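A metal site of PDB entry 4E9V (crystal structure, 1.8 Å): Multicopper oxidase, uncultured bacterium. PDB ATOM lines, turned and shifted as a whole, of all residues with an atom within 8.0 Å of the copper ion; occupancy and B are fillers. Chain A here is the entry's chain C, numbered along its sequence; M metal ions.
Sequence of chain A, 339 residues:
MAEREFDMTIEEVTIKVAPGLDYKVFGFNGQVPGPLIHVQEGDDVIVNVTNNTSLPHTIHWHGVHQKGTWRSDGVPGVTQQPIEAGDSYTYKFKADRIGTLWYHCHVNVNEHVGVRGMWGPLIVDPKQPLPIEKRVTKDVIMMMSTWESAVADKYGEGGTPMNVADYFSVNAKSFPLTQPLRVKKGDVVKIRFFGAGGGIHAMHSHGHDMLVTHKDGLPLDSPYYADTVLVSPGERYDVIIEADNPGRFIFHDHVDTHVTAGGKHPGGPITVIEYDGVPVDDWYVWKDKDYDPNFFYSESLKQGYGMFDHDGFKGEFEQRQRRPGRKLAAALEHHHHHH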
ATOM      1  N   ILE A  10      28.422  -3.030  -3.886  1.00  0.00           N
ATOM      2  CA  ILE A  10      27.953  -4.257  -4.537  1.00  0.00           C
ATOM      3  C   ILE A  10      29.183  -5.038  -4.981  1.00  0.00           C
ATOM      4  O   ILE A  10      30.042  -4.471  -5.654  1.00  0.00           O
ATOM      5  CB  ILE A  10      27.007  -3.940  -5.706  1.00  0.00           C
ATOM      6  CG1 ILE A  10      25.972  -2.866  -5.373  1.00  0.00           C
ATOM      7  CG2 ILE A  10      26.308  -5.200  -6.199  1.00  0.00           C
ATOM      8  CD1 ILE A  10      25.070  -2.471  -6.523  1.00  0.00           C
ATOM      9  N   PHE A  26      25.835 -11.403  -6.601  1.00  0.00           N
ATOM     10  CA  PHE A  26      26.176  -9.995  -6.434  1.00  0.00           C
ATOM     11  C   PHE A  26      25.765  -9.534  -5.035  1.00  0.00           C
ATOM     12  O   PHE A  26      24.665  -9.036  -4.797  1.00  0.00           O
ATOM     13  CB  PHE A  26      25.511  -9.104  -7.468  1.00  0.00           C
ATOM     14  CG  PHE A  26      25.846  -9.353  -8.918  1.00  0.00           C
ATOM     15  CD1 PHE A  26      27.099  -9.066  -9.419  1.00  0.00           C
ATOM     16  CD2 PHE A  26      24.890  -9.854  -9.786  1.00  0.00           C
ATOM     17  CE1 PHE A  26      27.388  -9.275 -10.753  1.00  0.00           C
ATOM     18  CE2 PHE A  26      25.153 -10.053 -11.138  1.00  0.00           C
ATOM     19  CZ  PHE A  26      26.423  -9.743 -11.608  1.00  0.00           C
ATOM     20  N   PHE A  28      25.408  -7.445  -1.735  1.00  0.00           N
ATOM     21  CA  PHE A  28      25.482  -6.154  -1.059  1.00  0.00           C
ATOM     22  C   PHE A  28      26.496  -6.263   0.076  1.00  0.00           C
ATOM     23  O   PHE A  28      26.360  -7.161   0.918  1.00  0.00           O
ATOM     24  CB  PHE A  28      24.100  -5.776  -0.542  1.00  0.00           C
ATOM     25  CG  PHE A  28      23.142  -5.376  -1.655  1.00  0.00           C
ATOM     26  CD1 PHE A  28      23.474  -4.351  -2.538  1.00  0.00           C
ATOM     27  CD2 PHE A  28      21.941  -6.044  -1.819  1.00  0.00           C
ATOM     28  CE1 PHE A  28      22.608  -3.972  -3.548  1.00  0.00           C
ATOM     29  CE2 PHE A  28      21.049  -5.659  -2.811  1.00  0.00           C
ATOM     30  CZ  PHE A  28      21.378  -4.634  -3.666  1.00  0.00           C
ATOM     31  N   ASN A  51      28.995   0.580  -7.036  1.00  0.00           N
ATOM     32  CA  ASN A  51      28.861  -0.640  -7.804  1.00  0.00           C
ATOM     33  C   ASN A  51      30.231  -1.208  -8.153  1.00  0.00           C
ATOM     34  O   ASN A  51      30.803  -0.785  -9.159  1.00  0.00           O
ATOM     35  CB  ASN A  51      28.052  -0.349  -9.072  1.00  0.00           C
ATOM     36  CG  ASN A  51      27.806  -1.600  -9.896  1.00  0.00           C
ATOM     37  OD1 ASN A  51      28.328  -2.678  -9.569  1.00  0.00           O
ATOM     38  ND2 ASN A  51      27.031  -1.462 -10.960  1.00  0.00           N
ATOM     39  N   THR A  53      30.836  -4.093  -9.220  1.00  0.00           N
ATOM     40  CA  THR A  53      30.729  -5.272 -10.084  1.00  0.00           C
ATOM     41  C   THR A  53      30.829  -4.855 -11.559  1.00  0.00           C
ATOM     42  O   THR A  53      30.950  -3.665 -11.810  1.00  0.00           O
ATOM     43  CB  THR A  53      29.431  -6.068  -9.861  1.00  0.00           C
ATOM     44  OG1 THR A  53      28.381  -5.469 -10.643  1.00  0.00           O
ATOM     45  CG2 THR A  53      29.026  -6.011  -8.392  1.00  0.00           C
ATOM     46  N   LEU A  55      28.459  -5.305 -13.815  1.00  0.00           N
ATOM     47  CA  LEU A  55      27.165  -5.131 -14.456  1.00  0.00           C
ATOM     48  C   LEU A  55      26.389  -4.039 -13.730  1.00  0.00           C
ATOM     49  O   LEU A  55      26.646  -3.743 -12.567  1.00  0.00           O
ATOM     50  CB  LEU A  55      26.343  -6.417 -14.457  1.00  0.00           C
ATOM     51  CG  LEU A  55      26.904  -7.649 -15.138  1.00  0.00           C
ATOM     52  CD1 LEU A  55      26.055  -8.875 -14.865  1.00  0.00           C
ATOM     53  CD2 LEU A  55      27.004  -7.423 -16.649  1.00  0.00           C
ATOM     54  N   PRO A  56      25.450  -3.409 -14.442  1.00  0.00           N
ATOM     55  CA  PRO A  56      24.656  -2.342 -13.825  1.00  0.00           C
ATOM     56  C   PRO A  56      23.648  -2.873 -12.805  1.00  0.00           C
ATOM     57  O   PRO A  56      23.126  -3.988 -12.963  1.00  0.00           O
ATOM     58  CB  PRO A  56      23.911  -1.745 -15.026  1.00  0.00           C
ATOM     59  CG  PRO A  56      24.013  -2.721 -16.143  1.00  0.00           C
ATOM     60  CD  PRO A  56      25.133  -3.667 -15.861  1.00  0.00           C
ATOM     61  N   HIS A  57      23.379  -2.116 -11.758  1.00  0.00           N
ATOM     62  CA  HIS A  57      22.379  -2.430 -10.744  1.00  0.00           C
ATOM     63  C   HIS A  57      21.624  -1.184 -10.292  1.00  0.00           C
ATOM     64  O   HIS A  57      21.978  -0.049 -10.638  1.00  0.00           O
ATOM     65  CB  HIS A  57      22.997  -3.095  -9.507  1.00  0.00           C
ATOM     66  CG  HIS A  57      23.902  -4.245  -9.820  1.00  0.00           C
ATOM     67  ND1 HIS A  57      23.481  -5.505 -10.152  1.00  0.00           N
ATOM     68  CD2 HIS A  57      25.265  -4.275  -9.882  1.00  0.00           C
ATOM     69  CE1 HIS A  57      24.537  -6.266 -10.388  1.00  0.00           C
ATOM     70  NE2 HIS A  57      25.633  -5.549 -10.237  1.00  0.00           N
ATOM     71  N   THR A  58      20.587  -1.394  -9.495  1.00  0.00           N
ATOM     72  CA  THR A  58      19.977  -0.357  -8.679  1.00  0.00           C
ATOM     73  C   THR A  58      19.687  -0.934  -7.292  1.00  0.00           C
ATOM     74  O   THR A  58      19.905  -2.126  -7.101  1.00  0.00           O
ATOM     75  CB  THR A  58      18.643   0.179  -9.223  1.00  0.00           C
ATOM     76  OG1 THR A  58      17.729  -0.925  -9.363  1.00  0.00           O
ATOM     77  CG2 THR A  58      18.824   0.782 -10.609  1.00  0.00           C
ATOM     78  N   ILE A  59      19.212  -0.110  -6.382  1.00  0.00           N
ATOM     79  CA  ILE A  59      18.586  -0.625  -5.176  1.00  0.00           C
ATOM     80  C   ILE A  59      17.187  -0.023  -5.051  1.00  0.00           C
ATOM     81  O   ILE A  59      17.004   1.208  -5.017  1.00  0.00           O
ATOM     82  CB  ILE A  59      19.351  -0.335  -3.875  1.00  0.00           C
ATOM     83  CG1 ILE A  59      20.813  -0.776  -3.914  1.00  0.00           C
ATOM     84  CG2 ILE A  59      18.583  -0.949  -2.707  1.00  0.00           C
ATOM     85  CD1 ILE A  59      21.588  -0.544  -2.641  1.00  0.00           C
ATOM     86  N   ILE A  83      22.758   2.234 -12.032  1.00  0.00           N
ATOM     87  CA  ILE A  83      24.108   2.513 -11.561  1.00  0.00           C
ATOM     88  C   ILE A  83      25.119   1.684 -12.308  1.00  0.00           C
ATOM     89  O   ILE A  83      25.252   0.463 -12.163  1.00  0.00           O
ATOM     90  CB  ILE A  83      24.288   2.212 -10.053  1.00  0.00           C
ATOM     91  CG1 ILE A  83      23.191   2.800  -9.175  1.00  0.00           C
ATOM     92  CG2 ILE A  83      25.677   2.655  -9.598  1.00  0.00           C
ATOM     93  CD1 ILE A  83      22.985   2.094  -7.849  1.00  0.00           C
ATOM     94  N   HIS A 104      16.118  -4.541  -2.646  1.00  0.00           N
ATOM     95  CA  HIS A 104      16.670  -5.461  -3.633  1.00  0.00           C
ATOM     96  C   HIS A 104      16.974  -4.770  -4.961  1.00  0.00           C
ATOM     97  O   HIS A 104      16.470  -3.674  -5.221  1.00  0.00           O
ATOM     98  CB  HIS A 104      15.696  -6.637  -3.858  1.00  0.00           C
ATOM     99  CG  HIS A 104      14.321  -6.246  -4.294  1.00  0.00           C
ATOM    100  ND1 HIS A 104      14.009  -5.933  -5.610  1.00  0.00           N
ATOM    101  CD2 HIS A 104      13.152  -6.166  -3.610  1.00  0.00           C
ATOM    102  CE1 HIS A 104      12.721  -5.648  -5.716  1.00  0.00           C
ATOM    103  NE2 HIS A 104      12.191  -5.785  -4.511  1.00  0.00           N
ATOM    104  N   CYS A 105      17.819  -5.417  -5.763  1.00  0.00           N
ATOM    105  CA  CYS A 105      18.152  -4.857  -7.081  1.00  0.00           C
ATOM    106  C   CYS A 105      16.885  -4.801  -7.940  1.00  0.00           C
ATOM    107  O   CYS A 105      15.987  -5.624  -7.763  1.00  0.00           O
ATOM    108  CB  CYS A 105      19.220  -5.670  -7.815  1.00  0.00           C
ATOM    109  SG  CYS A 105      19.765  -4.910  -9.364  1.00  0.00           S
ATOM    110  N   HIS A 106      16.801  -3.831  -8.843  1.00  0.00           N
ATOM    111  CA  HIS A 106      15.603  -3.793  -9.701  1.00  0.00           C
ATOM    112  C   HIS A 106      16.029  -3.737 -11.167  1.00  0.00           C
ATOM    113  O   HIS A 106      15.210  -3.426 -12.037  1.00  0.00           O
ATOM    114  CB  HIS A 106      14.712  -2.621  -9.330  1.00  0.00           C
ATOM    115  CG  HIS A 106      13.248  -2.892  -9.323  1.00  0.00           C
ATOM    116  ND1 HIS A 106      12.561  -3.182 -10.486  1.00  0.00           N
ATOM    117  CD2 HIS A 106      12.320  -2.925  -8.328  1.00  0.00           C
ATOM    118  CE1 HIS A 106      11.286  -3.378 -10.194  1.00  0.00           C
ATOM    119  NE2 HIS A 106      11.118  -3.239  -8.896  1.00  0.00           N
ATOM    120  N   VAL A 107      17.296  -4.049 -11.406  1.00  0.00           N
ATOM    121  CA  VAL A 107      17.835  -4.336 -12.740  1.00  0.00           C
ATOM    122  C   VAL A 107      17.824  -5.856 -12.961  1.00  0.00           C
ATOM    123  O   VAL A 107      18.330  -6.596 -12.108  1.00  0.00           O
ATOM    124  CB  VAL A 107      19.250  -3.796 -12.936  1.00  0.00           C
ATOM    125  CG1 VAL A 107      19.827  -4.217 -14.294  1.00  0.00           C
ATOM    126  CG2 VAL A 107      19.268  -2.271 -12.820  1.00  0.00           C
ATOM    127  N   ASN A 108      17.242  -6.290 -14.077  1.00  0.00           N
ATOM    128  CA  ASN A 108      17.233  -7.705 -14.447  1.00  0.00           C
ATOM    129  C   ASN A 108      16.775  -8.589 -13.287  1.00  0.00           C
ATOM    130  O   ASN A 108      17.475  -9.555 -12.961  1.00  0.00           O
ATOM    131  CB  ASN A 108      18.613  -8.166 -14.908  1.00  0.00           C
ATOM    132  CG  ASN A 108      18.931  -7.816 -16.343  1.00  0.00           C
ATOM    133  OD1 ASN A 108      18.122  -7.886 -17.263  1.00  0.00           O
ATOM    134  ND2 ASN A 108      20.179  -7.397 -16.552  1.00  0.00           N
ATOM    135  N   VAL A 109      15.646  -8.220 -12.691  1.00  0.00           N
ATOM    136  CA  VAL A 109      15.258  -8.784 -11.407  1.00  0.00           C
ATOM    137  C   VAL A 109      15.143 -10.302 -11.434  1.00  0.00           C
ATOM    138  O   VAL A 109      15.476 -10.941 -10.430  1.00  0.00           O
ATOM    139  CB  VAL A 109      13.956  -8.146 -10.886  1.00  0.00           C
ATOM    140  CG1 VAL A 109      14.067  -6.631 -10.924  1.00  0.00           C
ATOM    141  CG2 VAL A 109      12.764  -8.600 -11.689  1.00  0.00           C
ATOM    142  N   GLU A 111      16.958 -12.491 -12.692  1.00  0.00           N
ATOM    143  CA  GLU A 111      18.253 -13.091 -12.359  1.00  0.00           C
ATOM    144  C   GLU A 111      18.875 -12.482 -11.109  1.00  0.00           C
ATOM    145  O   GLU A 111      19.275 -13.268 -10.233  1.00  0.00           O
ATOM    146  CB  GLU A 111      19.263 -12.993 -13.508  1.00  0.00           C
ATOM    147  CG  GLU A 111      20.613 -13.589 -13.154  1.00  0.00           C
ATOM    148  CD  GLU A 111      21.756 -13.157 -14.052  1.00  0.00           C
ATOM    149  OE1 GLU A 111      21.558 -12.435 -15.061  1.00  0.00           O
ATOM    150  OE2 GLU A 111      22.917 -13.553 -13.740  1.00  0.00           O
ATOM    151  N   HIS A 112      18.974 -11.164 -11.035  1.00  0.00           N
ATOM    152  CA  HIS A 112      19.662 -10.506  -9.913  1.00  0.00           C
ATOM    153  C   HIS A 112      18.986 -10.822  -8.583  1.00  0.00           C
ATOM    154  O   HIS A 112      19.680 -11.157  -7.614  1.00  0.00           O
ATOM    155  CB  HIS A 112      19.727  -8.989 -10.105  1.00  0.00           C
ATOM    156  CG  HIS A 112      20.725  -8.616 -11.162  1.00  0.00           C
ATOM    157  ND1 HIS A 112      21.372  -7.397 -11.252  1.00  0.00           N
ATOM    158  CD2 HIS A 112      21.169  -9.404 -12.175  1.00  0.00           C
ATOM    159  CE1 HIS A 112      22.177  -7.476 -12.320  1.00  0.00           C
ATOM    160  NE2 HIS A 112      22.075  -8.664 -12.878  1.00  0.00           N
ATOM    161  N   VAL A 113      17.666 -10.737  -8.501  1.00  0.00           N
ATOM    162  CA  VAL A 113      17.007 -11.062  -7.227  1.00  0.00           C
ATOM    163  C   VAL A 113      16.709 -12.555  -7.168  1.00  0.00           C
ATOM    164  O   VAL A 113      16.769 -13.180  -6.110  1.00  0.00           O
ATOM    165  CB  VAL A 113      15.704 -10.277  -6.998  1.00  0.00           C
ATOM    166  CG1 VAL A 113      15.106 -10.481  -5.609  1.00  0.00           C
ATOM    167  CG2 VAL A 113      15.939  -8.781  -7.213  1.00  0.00           C
ATOM    168  N   ARG A 116      20.834 -14.184  -7.785  1.00  0.00           N
ATOM    169  CA  ARG A 116      22.140 -13.605  -7.474  1.00  0.00           C
ATOM    170  C   ARG A 116      22.204 -12.908  -6.125  1.00  0.00           C
ATOM    171  O   ARG A 116      23.145 -12.151  -5.856  1.00  0.00           O
ATOM    172  CB  ARG A 116      22.547 -12.644  -8.597  1.00  0.00           C
ATOM    173  CG  ARG A 116      22.562 -13.327  -9.958  1.00  0.00           C
ATOM    174  CD  ARG A 116      23.771 -14.244 -10.170  1.00  0.00           C
ATOM    175  NE  ARG A 116      23.542 -15.041 -11.375  1.00  0.00           N
ATOM    176  CZ  ARG A 116      23.936 -16.247 -11.704  1.00  0.00           C
ATOM    177  NH1 ARG A 116      24.696 -16.975 -10.879  1.00  0.00           N
ATOM    178  NH2 ARG A 116      23.602 -16.790 -12.877  1.00  0.00           N
ATOM    179  N   MET A 118      20.704 -10.503  -4.559  1.00  0.00           N
ATOM    180  CA  MET A 118      20.650  -9.050  -4.431  1.00  0.00           C
ATOM    181  C   MET A 118      19.477  -8.578  -3.590  1.00  0.00           C
ATOM    182  O   MET A 118      18.522  -7.934  -4.047  1.00  0.00           O
ATOM    183  CB  MET A 118      20.613  -8.422  -5.828  1.00  0.00           C
ATOM    184  CG  MET A 118      21.867  -8.745  -6.616  1.00  0.00           C
ATOM    185  SD  MET A 118      22.283  -7.492  -7.858  1.00  0.00           S
ATOM    186  CE  MET A 118      22.909  -6.159  -6.833  1.00  0.00           C
HETATM  187 CU    CU M   1      21.463  -6.135 -10.040  1.00  0.00          CU
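The backbone NH (N) of Val 107 sits close to the side-chain sulfur (SG) of Cys 105 (3.3 Å). A ring nitrogen (ND1) of His 112 sits close to the backbone carbonyl oxygen (O) of Val 107, at 3.3 Å. The side-chain sulfur (SG) of Cys 105 sits close to the backbone carbonyl oxygen (O) of Thr 58. O of Leu 55 sits close to NE2 of His 57, 3.1 Å away. The side-chain hydroxyl (OG1) of Thr 53 sits at hydrogen-bond distance from a ring nitrogen (NE2) of His 57, 2.8 Å away. The backbone carbonyl oxygen (O) of His 57 lies within hydrogen-bond range of the backbone NH (N) of Ile 83 (2.8 Å).
Merely in contact with the copper ion: Val 107 (3.8 Å) and Pro 56 (3.99 Å). Of the 22 residues printed, 6 come within 4 Å of the copper ion.
The copper ion is bound by ND1 of His 112 (1.8 Å), ND1 of His 57 (2.1 Å), SG of Cys 105 (2.2 Å) and SD of Met 118 (2.7 Å).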
